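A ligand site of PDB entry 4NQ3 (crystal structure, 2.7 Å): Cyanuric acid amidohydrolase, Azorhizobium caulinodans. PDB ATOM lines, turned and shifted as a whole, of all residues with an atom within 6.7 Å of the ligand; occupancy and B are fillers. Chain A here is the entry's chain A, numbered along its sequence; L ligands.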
ATOM      1  N   LYS A  40       7.665  -6.915 -19.511  1.00  0.00           N
ATOM      2  CA  LYS A  40       6.304  -7.246 -19.895  1.00  0.00           C
ATOM      3  C   LYS A  40       5.720  -7.983 -18.719  1.00  0.00           C
ATOM      4  O   LYS A  40       6.257  -9.002 -18.314  1.00  0.00           O
ATOM      5  CB  LYS A  40       6.277  -8.106 -21.155  1.00  0.00           C
ATOM      6  CG  LYS A  40       6.686  -7.370 -22.394  1.00  0.00           C
ATOM      7  CD  LYS A  40       5.828  -6.135 -22.564  1.00  0.00           C
ATOM      8  CE  LYS A  40       4.343  -6.489 -22.724  1.00  0.00           C
ATOM      9  NZ  LYS A  40       3.501  -5.256 -22.725  1.00  0.00           N
ATOM     10  N   THR A  41       4.657  -7.448 -18.121  1.00  0.00           N
ATOM     11  CA  THR A  41       4.057  -8.110 -16.956  1.00  0.00           C
ATOM     12  C   THR A  41       2.630  -8.591 -17.281  1.00  0.00           C
ATOM     13  O   THR A  41       1.984  -8.041 -18.169  1.00  0.00           O
ATOM     14  CB  THR A  41       4.071  -7.175 -15.745  1.00  0.00           C
ATOM     15  OG1 THR A  41       3.311  -5.992 -16.025  1.00  0.00           O
ATOM     16  CG2 THR A  41       5.501  -6.756 -15.452  1.00  0.00           C
ATOM     17  N   ASN A  44      -3.401  -6.481 -17.473  1.00  0.00           N
ATOM     18  CA  ASN A  44      -4.166  -6.263 -18.693  1.00  0.00           C
ATOM     19  C   ASN A  44      -3.613  -5.139 -19.544  1.00  0.00           C
ATOM     20  O   ASN A  44      -4.098  -4.901 -20.654  1.00  0.00           O
ATOM     21  CB  ASN A  44      -5.650  -6.028 -18.388  1.00  0.00           C
ATOM     22  CG  ASN A  44      -5.917  -4.799 -17.553  1.00  0.00           C
ATOM     23  OD1 ASN A  44      -5.062  -3.924 -17.407  1.00  0.00           O
ATOM     24  ND2 ASN A  44      -7.115  -4.719 -16.999  1.00  0.00           N
ATOM     25  N   GLY A  45      -2.580  -4.479 -19.023  1.00  0.00           N
ATOM     26  CA  GLY A  45      -1.927  -3.400 -19.736  1.00  0.00           C
ATOM     27  C   GLY A  45      -2.758  -2.127 -19.838  1.00  0.00           C
ATOM     28  O   GLY A  45      -2.406  -1.238 -20.604  1.00  0.00           O
ATOM     29  N   CYS A  46      -3.834  -2.005 -19.085  1.00  0.00           N
ATOM     30  CA  CYS A  46      -4.654  -0.805 -19.212  1.00  0.00           C
ATOM     31  C   CYS A  46      -4.687  -0.019 -17.908  1.00  0.00           C
ATOM     32  O   CYS A  46      -3.622   0.187 -17.284  1.00  0.00           O
ATOM     33  CB  CYS A  46      -6.061  -1.171 -19.688  1.00  0.00           C
ATOM     34  SG  CYS A  46      -6.005  -2.015 -21.331  1.00  0.00           S
ATOM     35  N   ASP A  49      -4.197  -2.118 -13.995  1.00  0.00           N
ATOM     36  CA  ASP A  49      -3.203  -3.147 -14.112  1.00  0.00           C
ATOM     37  C   ASP A  49      -2.212  -2.932 -12.990  1.00  0.00           C
ATOM     38  O   ASP A  49      -1.436  -1.993 -13.034  1.00  0.00           O
ATOM     39  CB  ASP A  49      -2.514  -3.080 -15.484  1.00  0.00           C
ATOM     40  CG  ASP A  49      -1.405  -4.127 -15.651  1.00  0.00           C
ATOM     41  OD1 ASP A  49      -0.868  -4.679 -14.628  1.00  0.00           O
ATOM     42  OD2 ASP A  49      -1.054  -4.390 -16.823  1.00  0.00           O
ATOM     43  N   ARG A  52       2.096  -4.162 -12.986  1.00  0.00           N
ATOM     44  CA  ARG A  52       3.157  -3.199 -13.274  1.00  0.00           C
ATOM     45  C   ARG A  52       3.774  -2.686 -11.977  1.00  0.00           C
ATOM     46  O   ARG A  52       4.989  -2.757 -11.767  1.00  0.00           O
ATOM     47  CB  ARG A  52       2.628  -2.013 -14.092  1.00  0.00           C
ATOM     48  CG  ARG A  52       2.251  -2.350 -15.534  1.00  0.00           C
ATOM     49  CD  ARG A  52       1.732  -1.158 -16.320  1.00  0.00           C
ATOM     50  NE  ARG A  52       0.668  -0.492 -15.593  1.00  0.00           N
ATOM     51  CZ  ARG A  52      -0.541  -0.254 -16.072  1.00  0.00           C
ATOM     52  NH1 ARG A  52      -0.853  -0.624 -17.307  1.00  0.00           N
ATOM     53  NH2 ARG A  52      -1.430   0.376 -15.317  1.00  0.00           N
ATOM     54  N   MET A  78       7.683  -0.770 -16.810  1.00  0.00           N
ATOM     55  CA  MET A  78       6.937  -2.014 -16.797  1.00  0.00           C
ATOM     56  C   MET A  78       5.723  -1.876 -17.691  1.00  0.00           C
ATOM     57  O   MET A  78       4.794  -1.137 -17.366  1.00  0.00           O
ATOM     58  CB  MET A  78       6.500  -2.399 -15.389  1.00  0.00           C
ATOM     59  CG  MET A  78       7.659  -2.680 -14.418  1.00  0.00           C
ATOM     60  SD  MET A  78       8.713  -4.245 -14.910  1.00  0.00           S
ATOM     61  CE  MET A  78      10.365  -3.309 -15.398  1.00  0.00           C
ATOM     62  N   SER A  79       5.748  -2.543 -18.832  1.00  0.00           N
ATOM     63  CA  SER A  79       4.613  -2.530 -19.749  1.00  0.00           C
ATOM     64  C   SER A  79       3.788  -3.775 -19.581  1.00  0.00           C
ATOM     65  O   SER A  79       4.303  -4.877 -19.795  1.00  0.00           O
ATOM     66  CB  SER A  79       5.072  -2.409 -21.189  1.00  0.00           C
ATOM     67  OG  SER A  79       3.946  -2.279 -22.028  1.00  0.00           O
ATOM     68  N   GLY A  80       2.538  -3.599 -19.157  1.00  0.00           N
ATOM     69  CA  GLY A  80       1.628  -4.702 -18.928  1.00  0.00           C
ATOM     70  C   GLY A  80       1.012  -5.203 -20.208  1.00  0.00           C
ATOM     71  O   GLY A  80       1.136  -4.581 -21.275  1.00  0.00           O
ATOM     72  N   GLY A  81       0.344  -6.350 -20.124  1.00  0.00           N
ATOM     73  CA  GLY A  81      -0.360  -6.890 -21.271  1.00  0.00           C
ATOM     74  C   GLY A  81       0.464  -7.912 -22.034  1.00  0.00           C
ATOM     75  O   GLY A  81       1.269  -7.537 -22.890  1.00  0.00           O
ATOM     76  N   LYS A 156       8.019   5.857 -20.246  1.00  0.00           N
ATOM     77  CA  LYS A 156       6.966   5.413 -19.350  1.00  0.00           C
ATOM     78  C   LYS A 156       6.241   6.655 -18.877  1.00  0.00           C
ATOM     79  O   LYS A 156       6.866   7.556 -18.334  1.00  0.00           O
ATOM     80  CB  LYS A 156       7.536   4.652 -18.168  1.00  0.00           C
ATOM     81  CG  LYS A 156       6.487   4.017 -17.303  1.00  0.00           C
ATOM     82  CD  LYS A 156       5.928   2.829 -17.978  1.00  0.00           C
ATOM     83  CE  LYS A 156       4.507   2.544 -17.552  1.00  0.00           C
ATOM     84  NZ  LYS A 156       3.900   1.456 -18.384  1.00  0.00           N
ATOM     85  N   CYS A 157       4.938   6.737 -19.120  1.00  0.00           N
ATOM     86  CA  CYS A 157       4.206   7.955 -18.775  1.00  0.00           C
ATOM     87  C   CYS A 157       2.993   7.657 -17.909  1.00  0.00           C
ATOM     88  O   CYS A 157       2.518   6.537 -17.879  1.00  0.00           O
ATOM     89  CB  CYS A 157       3.752   8.696 -20.031  1.00  0.00           C
ATOM     90  SG  CYS A 157       2.776   7.601 -21.113  1.00  0.00           S
ATOM     91  N   MET A 184      -4.754   7.379 -21.226  1.00  0.00           N
ATOM     92  CA  MET A 184      -3.549   6.614 -21.544  1.00  0.00           C
ATOM     93  C   MET A 184      -3.104   6.924 -22.963  1.00  0.00           C
ATOM     94  O   MET A 184      -1.901   7.035 -23.246  1.00  0.00           O
ATOM     95  CB  MET A 184      -3.771   5.110 -21.388  1.00  0.00           C
ATOM     96  CG  MET A 184      -4.084   4.681 -19.991  1.00  0.00           C
ATOM     97  SD  MET A 184      -3.937   2.751 -19.850  1.00  0.00           S
ATOM     98  CE  MET A 184      -5.767   2.238 -20.152  1.00  0.00           C
ATOM     99  N   ARG A 188       0.355   8.800 -23.900  1.00  0.00           N
ATOM    100  CA  ARG A 188       1.298   8.191 -24.832  1.00  0.00           C
ATOM    101  C   ARG A 188       1.544   9.158 -25.999  1.00  0.00           C
ATOM    102  O   ARG A 188       2.686   9.362 -26.420  1.00  0.00           O
ATOM    103  CB  ARG A 188       0.791   6.839 -25.381  1.00  0.00           C
ATOM    104  CG  ARG A 188       0.810   5.654 -24.428  1.00  0.00           C
ATOM    105  CD  ARG A 188       0.399   4.359 -25.134  1.00  0.00           C
ATOM    106  NE  ARG A 188      -0.962   4.477 -25.647  1.00  0.00           N
ATOM    107  CZ  ARG A 188      -2.028   3.893 -25.103  1.00  0.00           C
ATOM    108  NH1 ARG A 188      -1.876   3.116 -24.028  1.00  0.00           N
ATOM    109  NH2 ARG A 188      -3.234   4.063 -25.621  1.00  0.00           N
ATOM    110  N   CYS A 225       5.866   4.629 -26.402  1.00  0.00           N
ATOM    111  CA  CYS A 225       5.341   5.098 -25.128  1.00  0.00           C
ATOM    112  C   CYS A 225       4.407   4.114 -24.456  1.00  0.00           C
ATOM    113  O   CYS A 225       3.560   3.501 -25.115  1.00  0.00           O
ATOM    114  CB  CYS A 225       4.642   6.416 -25.348  1.00  0.00           C
ATOM    115  SG  CYS A 225       5.798   7.529 -26.133  1.00  0.00           S
ATOM    116  N   SER A 226       4.567   3.973 -23.152  1.00  0.00           N
ATOM    117  CA  SER A 226       3.821   3.018 -22.354  1.00  0.00           C
ATOM    118  C   SER A 226       3.315   3.735 -21.102  1.00  0.00           C
ATOM    119  O   SER A 226       4.104   4.329 -20.339  1.00  0.00           O
ATOM    120  CB  SER A 226       4.694   1.821 -21.994  1.00  0.00           C
ATOM    121  OG  SER A 226       4.023   0.912 -21.162  1.00  0.00           O
ATOM    122  N   SER A 227       2.004   3.721 -20.905  1.00  0.00           N
ATOM    123  CA  SER A 227       1.369   4.471 -19.840  1.00  0.00           C
ATOM    124  C   SER A 227       1.130   3.534 -18.646  1.00  0.00           C
ATOM    125  O   SER A 227       1.014   2.328 -18.809  1.00  0.00           O
ATOM    126  CB  SER A 227       0.073   5.112 -20.346  1.00  0.00           C
ATOM    127  OG  SER A 227      -0.523   5.981 -19.401  1.00  0.00           O
ATOM    128  N   GLY A 228       1.064   4.069 -17.424  1.00  0.00           N
ATOM    129  CA  GLY A 228       0.851   3.225 -16.283  1.00  0.00           C
ATOM    130  C   GLY A 228       0.310   3.979 -15.088  1.00  0.00           C
ATOM    131  O   GLY A 228       0.546   5.163 -14.925  1.00  0.00           O
ATOM    132  N   GLU A 230       1.124   3.546 -12.079  1.00  0.00           N
ATOM    133  CA  GLU A 230       2.053   3.477 -10.954  1.00  0.00           C
ATOM    134  C   GLU A 230       3.122   4.572 -10.872  1.00  0.00           C
ATOM    135  O   GLU A 230       4.019   4.479 -10.053  1.00  0.00           O
ATOM    136  CB  GLU A 230       2.786   2.134 -10.951  1.00  0.00           C
ATOM    137  CG  GLU A 230       3.698   1.865 -12.164  1.00  0.00           C
ATOM    138  CD  GLU A 230       2.883   1.356 -13.366  1.00  0.00           C
ATOM    139  OE1 GLU A 230       1.680   1.070 -13.147  1.00  0.00           O
ATOM    140  OE2 GLU A 230       3.433   1.170 -14.481  1.00  0.00           O
ATOM    141  N   LYS A 285       5.773  -1.480 -31.230  1.00  0.00           N
ATOM    142  CA  LYS A 285       4.486  -0.892 -30.881  1.00  0.00           C
ATOM    143  C   LYS A 285       3.378  -1.460 -31.766  1.00  0.00           C
ATOM    144  O   LYS A 285       3.537  -1.544 -32.973  1.00  0.00           O
ATOM    145  CB  LYS A 285       4.530   0.620 -31.032  1.00  0.00           C
ATOM    146  CG  LYS A 285       5.426   1.283 -30.040  1.00  0.00           C
ATOM    147  CD  LYS A 285       4.820   1.213 -28.663  1.00  0.00           C
ATOM    148  CE  LYS A 285       3.391   1.716 -28.675  1.00  0.00           C
ATOM    149  NZ  LYS A 285       2.834   1.600 -27.298  1.00  0.00           N
ATOM    150  N   THR A 310      -6.183  -2.086 -27.378  1.00  0.00           N
ATOM    151  CA  THR A 310      -4.760  -2.397 -27.300  1.00  0.00           C
ATOM    152  C   THR A 310      -4.484  -3.830 -26.914  1.00  0.00           C
ATOM    153  O   THR A 310      -3.464  -4.409 -27.308  1.00  0.00           O
ATOM    154  CB  THR A 310      -4.100  -1.549 -26.304  1.00  0.00           C
ATOM    155  OG1 THR A 310      -5.012  -1.376 -25.208  1.00  0.00           O
ATOM    156  CG2 THR A 310      -3.767  -0.224 -26.922  1.00  0.00           C
ATOM    157  N   ARG A 314      -2.023  -5.926 -29.292  1.00  0.00           N
ATOM    158  CA  ARG A 314      -0.846  -6.597 -28.751  1.00  0.00           C
ATOM    159  C   ARG A 314      -0.819  -8.074 -29.126  1.00  0.00           C
ATOM    160  O   ARG A 314       0.142  -8.538 -29.734  1.00  0.00           O
ATOM    161  CB  ARG A 314      -0.769  -6.448 -27.231  1.00  0.00           C
ATOM    162  CG  ARG A 314      -0.128  -5.178 -26.705  1.00  0.00           C
ATOM    163  CD  ARG A 314       0.156  -5.301 -25.200  1.00  0.00           C
ATOM    164  NE  ARG A 314      -1.063  -5.520 -24.444  1.00  0.00           N
ATOM    165  CZ  ARG A 314      -1.768  -4.545 -23.882  1.00  0.00           C
ATOM    166  NH1 ARG A 314      -1.326  -3.284 -23.965  1.00  0.00           N
ATOM    167  NH2 ARG A 314      -2.892  -4.825 -23.231  1.00  0.00           N
ATOM    168  N   TYR A 331       9.010  -7.932 -26.640  1.00  0.00           N
ATOM    169  CA  TYR A 331       8.406  -6.783 -25.976  1.00  0.00           C
ATOM    170  C   TYR A 331       7.470  -6.079 -26.954  1.00  0.00           C
ATOM    171  O   TYR A 331       7.921  -5.415 -27.873  1.00  0.00           O
ATOM    172  CB  TYR A 331       9.501  -5.831 -25.428  1.00  0.00           C
ATOM    173  CG  TYR A 331       8.966  -4.544 -24.804  1.00  0.00           C
ATOM    174  CD1 TYR A 331       8.524  -3.509 -25.605  1.00  0.00           C
ATOM    175  CD2 TYR A 331       8.917  -4.365 -23.421  1.00  0.00           C
ATOM    176  CE1 TYR A 331       8.034  -2.339 -25.066  1.00  0.00           C
ATOM    177  CE2 TYR A 331       8.421  -3.178 -22.880  1.00  0.00           C
ATOM    178  CZ  TYR A 331       7.974  -2.171 -23.722  1.00  0.00           C
ATOM    179  OH  TYR A 331       7.476  -0.972 -23.237  1.00  0.00           O
ATOM    180  N   VAL A 332       6.171  -6.293 -26.796  1.00  0.00           N
ATOM    181  CA  VAL A 332       5.165  -5.630 -27.617  1.00  0.00           C
ATOM    182  C   VAL A 332       4.241  -4.791 -26.769  1.00  0.00           C
ATOM    183  O   VAL A 332       3.669  -5.266 -25.815  1.00  0.00           O
ATOM    184  CB  VAL A 332       4.314  -6.641 -28.385  1.00  0.00           C
ATOM    185  CG1 VAL A 332       3.286  -5.922 -29.229  1.00  0.00           C
ATOM    186  CG2 VAL A 332       5.198  -7.532 -29.219  1.00  0.00           C
ATOM    187  N   SER A 333       4.042  -3.549 -27.181  1.00  0.00           N
ATOM    188  CA  SER A 333       3.356  -2.546 -26.387  1.00  0.00           C
ATOM    189  C   SER A 333       2.217  -1.939 -27.215  1.00  0.00           C
ATOM    190  O   SER A 333       2.396  -1.659 -28.388  1.00  0.00           O
ATOM    191  CB  SER A 333       4.361  -1.483 -25.950  1.00  0.00           C
ATOM    192  OG  SER A 333       3.702  -0.374 -25.409  1.00  0.00           O
ATOM    193  N   GLY A 334       1.037  -1.760 -26.620  1.00  0.00           N
ATOM    194  CA  GLY A 334      -0.132  -1.353 -27.384  1.00  0.00           C
ATOM    195  C   GLY A 334      -0.381   0.143 -27.393  1.00  0.00           C
ATOM    196  O   GLY A 334       0.036   0.836 -26.480  1.00  0.00           O
ATOM    197  N   GLY A 335      -1.052   0.641 -28.423  1.00  0.00           N
ATOM    198  CA  GLY A 335      -1.416   2.053 -28.507  1.00  0.00           C
ATOM    199  C   GLY A 335      -0.295   2.882 -29.112  1.00  0.00           C
ATOM    200  O   GLY A 335       0.674   3.227 -28.435  1.00  0.00           O
HETATM  201  N1  LIG L   1       0.633   0.425 -20.842  1.00  0.00           N
HETATM  202  C1  LIG L   1       0.890  -0.882 -20.598  1.00  0.00           C
HETATM  203  O1  LIG L   1       0.927  -1.247 -19.443  1.00  0.00           O
HETATM  204  N2  LIG L   1       1.093  -1.748 -21.629  1.00  0.00           N
HETATM  205  C2  LIG L   1       1.038  -1.335 -22.981  1.00  0.00           C
HETATM  206  O2  LIG L   1       1.214  -2.151 -23.885  1.00  0.00           O
HETATM  207  C3  LIG L   1       0.792   0.123 -23.387  1.00  0.00           C
HETATM  208  C4  LIG L   1       0.585   0.943 -22.132  1.00  0.00           C
HETATM  209  O3  LIG L   1       0.352   2.138 -22.232  1.00  0.00           O
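N of Ser 227 lies within hydrogen-bond range of O3 of the ligand (2.6 Å). The backbone carbonyl oxygen of Ser 227 is in hydrogen-bond range of a nitrogen (N1) of the ligand (2.8 Å). The backbone NH (N) of Gly 334 lies within hydrogen-bond range of an oxygen (O2) of the ligand (2.8 Å). The guanidinium group of Arg 314 is in hydrogen-bond range of an oxygen (O2) of the ligand (2.8 Å). An oxygen (O1) of the ligand is in hydrogen-bond range of the guanidinium group (NH1) of Arg 52 (2.8 Å). O1 of the ligand sits at hydrogen-bond distance from N of Gly 80 (2.9 Å). The backbone carbonyl oxygen of Gly 80 sits at hydrogen-bond distance from a nitrogen (N2) of the ligand (2.9 Å). A nitrogen (N2) of the ligand sits at hydrogen-bond distance from the side-chain hydroxyl (OG) of Ser 79, 2.9 Å away. The guanidinium group of Arg 188 sits at hydrogen-bond distance from an oxygen (O3) of the ligand, at 3.0 Å. N1 of the ligand sits close to O of Gly 45 (3.5 Å). An oxygen (O2) of the ligand sits close to the side-chain hydroxyl (OG) of Ser 333. The side-chain hydroxyl (OG) of Ser 226 lies within hydrogen-bond range of a nitrogen (N1) of the ligand (3.4 Å).
The nearest printed residue that does not touch the ligand is Lys 40 (4.03 Å).
NZ of Lys 156 sits at hydrogen-bond distance from O of Ser 227. O of Gly 81 sits close to NE of Arg 314, at 3.5 Å. NH1 of Arg 52 lies within salt-bridge range of OD2 of Asp 49 (3.8 Å). The backbone carbonyl oxygen (O) of Gly 80 sits at hydrogen-bond distance from the side-chain amino group (NZ) of Lys 40, 2.9 Å away. The backbone carbonyl oxygen (O) of Ser 79 is in hydrogen-bond range of the backbone NH (N) of Thr 41 (3.1 Å). The backbone carbonyl oxygen (O) of Gly 335 is in hydrogen-bond range of the guanidinium group (NE) of Arg 188 (3.5 Å). The side-chain carboxylate (OD2) of Asp 49 is in hydrogen-bond range of the backbone NH (N) of Gly 45, at 2.7 Å. The backbone carbonyl oxygen of Ser 226 sits at hydrogen-bond distance from the backbone NH of Cys 157, 2.8 Å away.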
